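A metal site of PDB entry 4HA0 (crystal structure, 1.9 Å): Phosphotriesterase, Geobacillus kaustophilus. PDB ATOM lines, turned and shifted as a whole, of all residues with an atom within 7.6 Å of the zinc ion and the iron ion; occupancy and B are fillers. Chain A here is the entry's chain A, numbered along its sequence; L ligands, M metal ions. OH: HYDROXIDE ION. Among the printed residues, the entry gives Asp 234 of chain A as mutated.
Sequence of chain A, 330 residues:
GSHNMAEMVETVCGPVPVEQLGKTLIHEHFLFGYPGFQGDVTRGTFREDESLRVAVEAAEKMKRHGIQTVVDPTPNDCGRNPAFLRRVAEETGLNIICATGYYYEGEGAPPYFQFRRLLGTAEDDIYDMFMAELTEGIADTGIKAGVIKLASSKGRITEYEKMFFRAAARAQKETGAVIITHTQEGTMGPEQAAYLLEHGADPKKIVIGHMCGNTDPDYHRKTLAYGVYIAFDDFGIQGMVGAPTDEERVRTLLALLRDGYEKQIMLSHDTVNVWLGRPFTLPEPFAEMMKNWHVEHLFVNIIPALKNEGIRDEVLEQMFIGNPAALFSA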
ATOM      1  N   HIS A  27       5.884 -29.832 -32.448  1.00  0.00           N
ATOM      2  CA  HIS A  27       6.850 -28.786 -32.129  1.00  0.00           C
ATOM      3  C   HIS A  27       6.856 -27.614 -33.125  1.00  0.00           C
ATOM      4  O   HIS A  27       7.481 -27.713 -34.173  1.00  0.00           O
ATOM      5  CB  HIS A  27       8.260 -29.394 -32.064  1.00  0.00           C
ATOM      6  CG  HIS A  27       9.260 -28.557 -31.333  1.00  0.00           C
ATOM      7  ND1 HIS A  27      10.027 -29.073 -30.308  1.00  0.00           N
ATOM      8  CD2 HIS A  27       9.654 -27.276 -31.482  1.00  0.00           C
ATOM      9  CE1 HIS A  27      10.842 -28.140 -29.845  1.00  0.00           C
ATOM     10  NE2 HIS A  27      10.624 -27.037 -30.533  1.00  0.00           N
ATOM     11  N   GLU A  28       6.155 -26.529 -32.784  1.00  0.00           N
ATOM     12  CA  GLU A  28       6.149 -25.287 -33.565  1.00  0.00           C
ATOM     13  C   GLU A  28       6.046 -24.104 -32.602  1.00  0.00           C
ATOM     14  O   GLU A  28       5.512 -24.276 -31.495  1.00  0.00           O
ATOM     15  CB  GLU A  28       4.970 -25.270 -34.538  1.00  0.00           C
ATOM     16  CG  GLU A  28       4.757 -26.562 -35.340  1.00  0.00           C
ATOM     17  CD  GLU A  28       5.705 -26.697 -36.520  1.00  0.00           C
ATOM     18  OE1 GLU A  28       6.286 -25.672 -36.938  1.00  0.00           O
ATOM     19  OE2 GLU A  28       5.870 -27.834 -37.029  1.00  0.00           O
ATOM     20  N   HIS A  29       6.549 -22.923 -32.992  1.00  0.00           N
ATOM     21  CA  HIS A  29       6.374 -21.692 -32.200  1.00  0.00           C
ATOM     22  C   HIS A  29       5.554 -20.652 -32.927  1.00  0.00           C
ATOM     23  O   HIS A  29       5.946 -20.205 -34.016  1.00  0.00           O
ATOM     24  CB  HIS A  29       7.725 -21.039 -31.888  1.00  0.00           C
ATOM     25  CG  HIS A  29       8.654 -21.927 -31.153  1.00  0.00           C
ATOM     26  ND1 HIS A  29       8.693 -21.977 -29.780  1.00  0.00           N
ATOM     27  CD2 HIS A  29       9.587 -22.804 -31.588  1.00  0.00           C
ATOM     28  CE1 HIS A  29       9.584 -22.869 -29.396  1.00  0.00           C
ATOM     29  NE2 HIS A  29      10.152 -23.374 -30.473  1.00  0.00           N
ATOM     30  N   PHE A  32       8.391 -16.444 -30.780  1.00  0.00           N
ATOM     31  CA  PHE A  32       9.680 -16.797 -30.169  1.00  0.00           C
ATOM     32  C   PHE A  32      10.624 -15.588 -30.174  1.00  0.00           C
ATOM     33  O   PHE A  32      10.768 -14.926 -31.185  1.00  0.00           O
ATOM     34  CB  PHE A  32      10.356 -17.945 -30.904  1.00  0.00           C
ATOM     35  CG  PHE A  32      11.595 -18.474 -30.212  1.00  0.00           C
ATOM     36  CD1 PHE A  32      12.838 -17.865 -30.410  1.00  0.00           C
ATOM     37  CD2 PHE A  32      11.521 -19.588 -29.380  1.00  0.00           C
ATOM     38  CE1 PHE A  32      13.989 -18.339 -29.777  1.00  0.00           C
ATOM     39  CE2 PHE A  32      12.670 -20.070 -28.735  1.00  0.00           C
ATOM     40  CZ  PHE A  32      13.904 -19.457 -28.933  1.00  0.00           C
ATOM     41  N   ASP A  72       3.181 -26.187 -28.604  1.00  0.00           N
ATOM     42  CA  ASP A  72       4.059 -25.017 -28.688  1.00  0.00           C
ATOM     43  C   ASP A  72       4.905 -24.962 -27.426  1.00  0.00           C
ATOM     44  O   ASP A  72       4.428 -24.541 -26.377  1.00  0.00           O
ATOM     45  CB  ASP A  72       3.217 -23.752 -28.824  1.00  0.00           C
ATOM     46  CG  ASP A  72       4.066 -22.478 -28.970  1.00  0.00           C
ATOM     47  OD1 ASP A  72       5.196 -22.467 -28.453  1.00  0.00           O
ATOM     48  OD2 ASP A  72       3.591 -21.518 -29.591  1.00  0.00           O
ATOM     49  N   PRO A  73       6.167 -25.404 -27.520  1.00  0.00           N
ATOM     50  CA  PRO A  73       7.027 -25.518 -26.338  1.00  0.00           C
ATOM     51  C   PRO A  73       7.978 -24.330 -26.199  1.00  0.00           C
ATOM     52  O   PRO A  73       9.142 -24.515 -25.790  1.00  0.00           O
ATOM     53  CB  PRO A  73       7.839 -26.764 -26.648  1.00  0.00           C
ATOM     54  CG  PRO A  73       8.065 -26.664 -28.148  1.00  0.00           C
ATOM     55  CD  PRO A  73       6.822 -25.974 -28.709  1.00  0.00           C
ATOM     56  N   THR A  74       7.505 -23.139 -26.547  1.00  0.00           N
ATOM     57  CA  THR A  74       8.280 -21.929 -26.331  1.00  0.00           C
ATOM     58  C   THR A  74       8.659 -21.842 -24.851  1.00  0.00           C
ATOM     59  O   THR A  74       7.794 -21.898 -23.988  1.00  0.00           O
ATOM     60  CB  THR A  74       7.484 -20.666 -26.715  1.00  0.00           C
ATOM     61  OG1 THR A  74       7.067 -20.748 -28.091  1.00  0.00           O
ATOM     62  CG2 THR A  74       8.323 -19.418 -26.491  1.00  0.00           C
ATOM     63  N   PRO A  75       9.967 -21.770 -24.564  1.00  0.00           N
ATOM     64  CA  PRO A  75      10.483 -21.669 -23.192  1.00  0.00           C
ATOM     65  C   PRO A  75      10.004 -20.417 -22.472  1.00  0.00           C
ATOM     66  O   PRO A  75       9.814 -19.397 -23.111  1.00  0.00           O
ATOM     67  CB  PRO A  75      12.008 -21.572 -23.400  1.00  0.00           C
ATOM     68  CG  PRO A  75      12.268 -22.255 -24.713  1.00  0.00           C
ATOM     69  CD  PRO A  75      11.052 -21.915 -25.564  1.00  0.00           C
ATOM     70  N   TYR A 103      15.066 -22.451 -21.433  1.00  0.00           N
ATOM     71  CA  TYR A 103      15.926 -22.885 -22.511  1.00  0.00           C
ATOM     72  C   TYR A 103      17.287 -23.331 -22.026  1.00  0.00           C
ATOM     73  O   TYR A 103      17.560 -23.276 -20.865  1.00  0.00           O
ATOM     74  CB  TYR A 103      16.108 -21.783 -23.546  1.00  0.00           C
ATOM     75  CG  TYR A 103      16.070 -22.154 -24.993  1.00  0.00           C
ATOM     76  CD1 TYR A 103      15.462 -23.299 -25.449  1.00  0.00           C
ATOM     77  CD2 TYR A 103      16.659 -21.343 -25.920  1.00  0.00           C
ATOM     78  CE1 TYR A 103      15.424 -23.590 -26.775  1.00  0.00           C
ATOM     79  CE2 TYR A 103      16.634 -21.652 -27.245  1.00  0.00           C
ATOM     80  CZ  TYR A 103      16.007 -22.771 -27.672  1.00  0.00           C
ATOM     81  OH  TYR A 103      15.955 -23.066 -28.996  1.00  0.00           O
ATOM     82  N   TYR A 104      18.077 -23.805 -22.959  1.00  0.00           N
ATOM     83  CA  TYR A 104      19.420 -24.248 -22.676  1.00  0.00           C
ATOM     84  C   TYR A 104      20.322 -23.086 -22.325  1.00  0.00           C
ATOM     85  O   TYR A 104      20.029 -22.008 -22.636  1.00  0.00           O
ATOM     86  CB  TYR A 104      19.999 -25.113 -23.775  1.00  0.00           C
ATOM     87  CG  TYR A 104      20.494 -24.445 -25.038  1.00  0.00           C
ATOM     88  CD1 TYR A 104      19.656 -24.140 -26.056  1.00  0.00           C
ATOM     89  CD2 TYR A 104      21.856 -24.206 -25.217  1.00  0.00           C
ATOM     90  CE1 TYR A 104      20.125 -23.579 -27.180  1.00  0.00           C
ATOM     91  CE2 TYR A 104      22.318 -23.657 -26.359  1.00  0.00           C
ATOM     92  CZ  TYR A 104      21.455 -23.341 -27.325  1.00  0.00           C
ATOM     93  OH  TYR A 104      21.932 -22.808 -28.455  1.00  0.00           O
ATOM     94  N   KCX A 149       9.071 -28.399 -20.897  1.00  0.00           N
ATOM     95  CA  KCX A 149      10.135 -28.271 -21.882  1.00  0.00           C
ATOM     96  CB  KCX A 149       9.965 -26.973 -22.674  1.00  0.00           C
ATOM     97  CG  KCX A 149      11.150 -26.584 -23.576  1.00  0.00           C
ATOM     98  CD  KCX A 149      11.474 -27.678 -24.575  1.00  0.00           C
ATOM     99  CE  KCX A 149      12.306 -27.150 -25.713  1.00  0.00           C
ATOM    100  NZ  KCX A 149      11.692 -25.991 -26.417  1.00  0.00           N
ATOM    101  C   KCX A 149      11.515 -28.330 -21.210  1.00  0.00           C
ATOM    102  O   KCX A 149      11.804 -27.571 -20.280  1.00  0.00           O
ATOM    103  CX  KCX A 149      12.117 -25.712 -27.649  1.00  0.00           C
ATOM    104  OQ1 KCX A 149      11.670 -24.761 -28.301  1.00  0.00           O
ATOM    105  OQ2 KCX A 149      12.979 -26.438 -28.128  1.00  0.00           O
ATOM    106  N   LEU A 150      12.351 -29.245 -21.680  1.00  0.00           N
ATOM    107  CA  LEU A 150      13.740 -29.316 -21.220  1.00  0.00           C
ATOM    108  C   LEU A 150      14.714 -28.996 -22.374  1.00  0.00           C
ATOM    109  O   LEU A 150      14.387 -29.228 -23.536  1.00  0.00           O
ATOM    110  CB  LEU A 150      14.047 -30.701 -20.655  1.00  0.00           C
ATOM    111  CG  LEU A 150      13.387 -31.099 -19.341  1.00  0.00           C
ATOM    112  CD1 LEU A 150      13.853 -32.512 -18.931  1.00  0.00           C
ATOM    113  CD2 LEU A 150      13.702 -30.074 -18.258  1.00  0.00           C
ATOM    114  N   ALA A 151      15.891 -28.470 -22.056  1.00  0.00           N
ATOM    115  CA  ALA A 151      16.834 -28.151 -23.115  1.00  0.00           C
ATOM    116  C   ALA A 151      18.255 -28.343 -22.622  1.00  0.00           C
ATOM    117  O   ALA A 151      18.551 -28.061 -21.454  1.00  0.00           O
ATOM    118  CB  ALA A 151      16.610 -26.720 -23.584  1.00  0.00           C
ATOM    119  N   THR A 181      11.906 -32.373 -25.178  1.00  0.00           N
ATOM    120  CA  THR A 181      13.248 -31.795 -25.047  1.00  0.00           C
ATOM    121  C   THR A 181      13.760 -31.135 -26.310  1.00  0.00           C
ATOM    122  O   THR A 181      13.261 -31.382 -27.400  1.00  0.00           O
ATOM    123  CB  THR A 181      14.278 -32.836 -24.617  1.00  0.00           C
ATOM    124  OG1 THR A 181      14.683 -33.622 -25.749  1.00  0.00           O
ATOM    125  CG2 THR A 181      13.697 -33.753 -23.574  1.00  0.00           C
ATOM    126  N   HIS A 182      14.770 -30.282 -26.121  1.00  0.00           N
ATOM    127  CA  HIS A 182      15.604 -29.732 -27.200  1.00  0.00           C
ATOM    128  C   HIS A 182      17.022 -30.307 -27.060  1.00  0.00           C
ATOM    129  O   HIS A 182      17.616 -30.275 -25.970  1.00  0.00           O
ATOM    130  CB  HIS A 182      15.628 -28.202 -27.111  1.00  0.00           C
ATOM    131  CG  HIS A 182      16.869 -27.547 -27.660  1.00  0.00           C
ATOM    132  ND1 HIS A 182      16.852 -26.708 -28.749  1.00  0.00           N
ATOM    133  CD2 HIS A 182      18.156 -27.574 -27.236  1.00  0.00           C
ATOM    134  CE1 HIS A 182      18.064 -26.249 -28.984  1.00  0.00           C
ATOM    135  NE2 HIS A 182      18.884 -26.760 -28.087  1.00  0.00           N
ATOM    136  N   THR A 183      17.563 -30.844 -28.139  1.00  0.00           N
ATOM    137  CA  THR A 183      18.974 -31.218 -28.147  1.00  0.00           C
ATOM    138  C   THR A 183      19.733 -30.269 -29.041  1.00  0.00           C
ATOM    139  O   THR A 183      19.234 -29.865 -30.089  1.00  0.00           O
ATOM    140  CB  THR A 183      19.220 -32.691 -28.609  1.00  0.00           C
ATOM    141  OG1 THR A 183      18.648 -32.911 -29.918  1.00  0.00           O
ATOM    142  CG2 THR A 183      18.638 -33.652 -27.621  1.00  0.00           C
ATOM    143  N   GLN A 184      20.954 -29.909 -28.643  1.00  0.00           N
ATOM    144  CA  GLN A 184      21.691 -28.902 -29.411  1.00  0.00           C
ATOM    145  C   GLN A 184      22.662 -29.549 -30.379  1.00  0.00           C
ATOM    146  O   GLN A 184      23.467 -30.412 -30.001  1.00  0.00           O
ATOM    147  CB  GLN A 184      22.427 -27.940 -28.466  1.00  0.00           C
ATOM    148  CG  GLN A 184      23.160 -26.810 -29.189  1.00  0.00           C
ATOM    149  CD  GLN A 184      22.217 -25.780 -29.809  1.00  0.00           C
ATOM    150  OE1 GLN A 184      21.034 -25.715 -29.478  1.00  0.00           O
ATOM    151  NE2 GLN A 184      22.755 -24.962 -30.712  1.00  0.00           N
ATOM    152  N   GLY A 209      13.867 -34.170 -28.570  1.00  0.00           N
ATOM    153  CA  GLY A 209      13.682 -33.347 -29.751  1.00  0.00           C
ATOM    154  C   GLY A 209      14.931 -33.129 -30.565  1.00  0.00           C
ATOM    155  O   GLY A 209      16.044 -33.441 -30.123  1.00  0.00           O
ATOM    156  N   HIS A 210      14.753 -32.584 -31.769  1.00  0.00           N
ATOM    157  CA  HIS A 210      15.858 -32.221 -32.659  1.00  0.00           C
ATOM    158  C   HIS A 210      16.816 -33.379 -32.905  1.00  0.00           C
ATOM    159  O   HIS A 210      18.022 -33.186 -33.072  1.00  0.00           O
ATOM    160  CB  HIS A 210      16.605 -31.003 -32.116  1.00  0.00           C
ATOM    161  CG  HIS A 210      15.691 -29.878 -31.758  1.00  0.00           C
ATOM    162  ND1 HIS A 210      14.435 -29.755 -32.311  1.00  0.00           N
ATOM    163  CD2 HIS A 210      15.821 -28.850 -30.890  1.00  0.00           C
ATOM    164  CE1 HIS A 210      13.841 -28.694 -31.816  1.00  0.00           C
ATOM    165  NE2 HIS A 210      14.654 -28.135 -30.955  1.00  0.00           N
ATOM    166  N   ASP A 233      11.859 -32.747 -35.812  1.00  0.00           N
ATOM    167  CA  ASP A 233      10.996 -31.572 -35.649  1.00  0.00           C
ATOM    168  C   ASP A 233      11.561 -30.293 -36.253  1.00  0.00           C
ATOM    169  O   ASP A 233      11.011 -29.212 -36.019  1.00  0.00           O
ATOM    170  CB  ASP A 233      10.755 -31.362 -34.160  1.00  0.00           C
ATOM    171  CG  ASP A 233      12.042 -31.396 -33.359  1.00  0.00           C
ATOM    172  OD1 ASP A 233      13.114 -31.149 -33.935  1.00  0.00           O
ATOM    173  OD2 ASP A 233      11.969 -31.705 -32.151  1.00  0.00           O
ATOM    174  N   ASP A 234      12.650 -30.403 -37.004  1.00  0.00           N
ATOM    175  CA  ASP A 234      13.316 -29.241 -37.552  1.00  0.00           C
ATOM    176  C   ASP A 234      13.220 -29.158 -39.076  1.00  0.00           C
ATOM    177  O   ASP A 234      14.065 -28.529 -39.711  1.00  0.00           O
ATOM    178  CB  ASP A 234      14.811 -29.252 -37.162  1.00  0.00           C
ATOM    179  CG  ASP A 234      15.076 -28.594 -35.820  1.00  0.00           C
ATOM    180  OD1 ASP A 234      14.283 -27.724 -35.419  1.00  0.00           O
ATOM    181  OD2 ASP A 234      16.081 -28.961 -35.176  1.00  0.00           O
ATOM    182  N   HIS A 269       8.248 -28.865 -37.710  1.00  0.00           N
ATOM    183  CA  HIS A 269       9.130 -27.892 -38.346  1.00  0.00           C
ATOM    184  C   HIS A 269       9.925 -27.015 -37.396  1.00  0.00           C
ATOM    185  O   HIS A 269      10.943 -26.461 -37.805  1.00  0.00           O
ATOM    186  CB  HIS A 269       8.341 -26.957 -39.244  1.00  0.00           C
ATOM    187  CG  HIS A 269       7.403 -27.650 -40.184  1.00  0.00           C
ATOM    188  ND1 HIS A 269       6.084 -27.882 -39.858  1.00  0.00           N
ATOM    189  CD2 HIS A 269       7.579 -28.122 -41.437  1.00  0.00           C
ATOM    190  CE1 HIS A 269       5.484 -28.473 -40.879  1.00  0.00           C
ATOM    191  NE2 HIS A 269       6.375 -28.629 -41.846  1.00  0.00           N
ATOM    192  N   ASP A 270       9.455 -26.865 -36.158  1.00  0.00           N
ATOM    193  CA  ASP A 270      10.078 -25.928 -35.218  1.00  0.00           C
ATOM    194  C   ASP A 270      10.020 -24.492 -35.766  1.00  0.00           C
ATOM    195  O   ASP A 270      10.937 -23.695 -35.518  1.00  0.00           O
ATOM    196  CB  ASP A 270      11.533 -26.344 -34.981  1.00  0.00           C
ATOM    197  CG  ASP A 270      12.145 -25.677 -33.769  1.00  0.00           C
ATOM    198  OD1 ASP A 270      11.388 -25.101 -32.986  1.00  0.00           O
ATOM    199  OD2 ASP A 270      13.372 -25.737 -33.608  1.00  0.00           O
ATOM    200  N   THR A 271       8.972 -24.159 -36.522  1.00  0.00           N
ATOM    201  CA  THR A 271       8.841 -22.802 -37.083  1.00  0.00           C
ATOM    202  C   THR A 271       8.773 -21.737 -35.995  1.00  0.00           C
ATOM    203  O   THR A 271       8.369 -22.011 -34.857  1.00  0.00           O
ATOM    204  CB  THR A 271       7.593 -22.636 -37.977  1.00  0.00           C
ATOM    205  OG1 THR A 271       6.391 -22.889 -37.234  1.00  0.00           O
ATOM    206  CG2 THR A 271       7.637 -23.534 -39.197  1.00  0.00           C
ATOM    207  N   VAL A 272       9.146 -20.507 -36.348  1.00  0.00           N
ATOM    208  CA  VAL A 272       8.869 -19.348 -35.535  1.00  0.00           C
ATOM    209  C   VAL A 272       8.090 -18.439 -36.430  1.00  0.00           C
ATOM    210  O   VAL A 272       8.575 -18.011 -37.445  1.00  0.00           O
ATOM    211  CB  VAL A 272      10.150 -18.622 -35.083  1.00  0.00           C
ATOM    212  CG1 VAL A 272       9.785 -17.416 -34.257  1.00  0.00           C
ATOM    213  CG2 VAL A 272      11.018 -19.547 -34.286  1.00  0.00           C
HETATM  214  O    OH L   1      13.882 -24.713 -31.205  1.00  0.00           O
HETATM  215 ZN    ZN M   1      14.669 -26.315 -29.605  1.00  0.00          ZN
HETATM  216 FE    FE M   2      11.687 -25.043 -30.619  1.00  0.00          FE
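The iron ion is bound by a ring nitrogen (NE2) of His 27.
NE2 of His 29 binds the iron ion (2.3 Å).
An oxygen (O) of the ligand binds the iron ion, 2.3 Å away.
OQ1 of KCX 149 binds the iron ion (2.3 Å).
The iron ion is bound by OD1 of Asp 270 (2.4 Å).
Tyr 103 touches the zinc ion (OH to ZN, 3.5 Å).
Of the 25 residues printed, 4 come within 4 Å of the zinc ion.
The nearest printed residue that does not touch the zinc ion is His 27 (4.2 Å).
OQ2 of KCX 149 binds the zinc ion.
The zinc ion is bound by a ring nitrogen (NE2) of His 210 (2.3 Å).
The zinc ion is bound by ND1 of His 182 (2.4 Å).
O of the ligand is bound to the zinc ion, 2.4 Å away.
The nearest printed residue that does not touch the iron ion is His 210 (4.3 Å).
NZ of KCX 149 sits at hydrogen-bond distance from O of Pro 73.
O of His 210 is in hydrogen-bond range of OG1 of Thr 183 (3.2 Å).
A ring nitrogen (ND1) of His 210 lies within hydrogen-bond range of the side-chain carboxylate (OD2) of Asp 234 (3.4 Å).
A ring nitrogen (ND1) of His 210 lies within hydrogen-bond range of the side-chain carboxylate of Asp 233, 2.5 Å away.
OG1 of Thr 74 lies within hydrogen-bond range of ND1 of His 29.
The backbone carbonyl oxygen (O) of Thr 271 sits at hydrogen-bond distance from the backbone NH (N) of His 29 (2.8 Å).
N of His 182 is in hydrogen-bond range of O of Leu 150, at 2.8 Å.
N of Asp 270 lies within hydrogen-bond range of OE1 of Glu 28 (3.5 Å).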
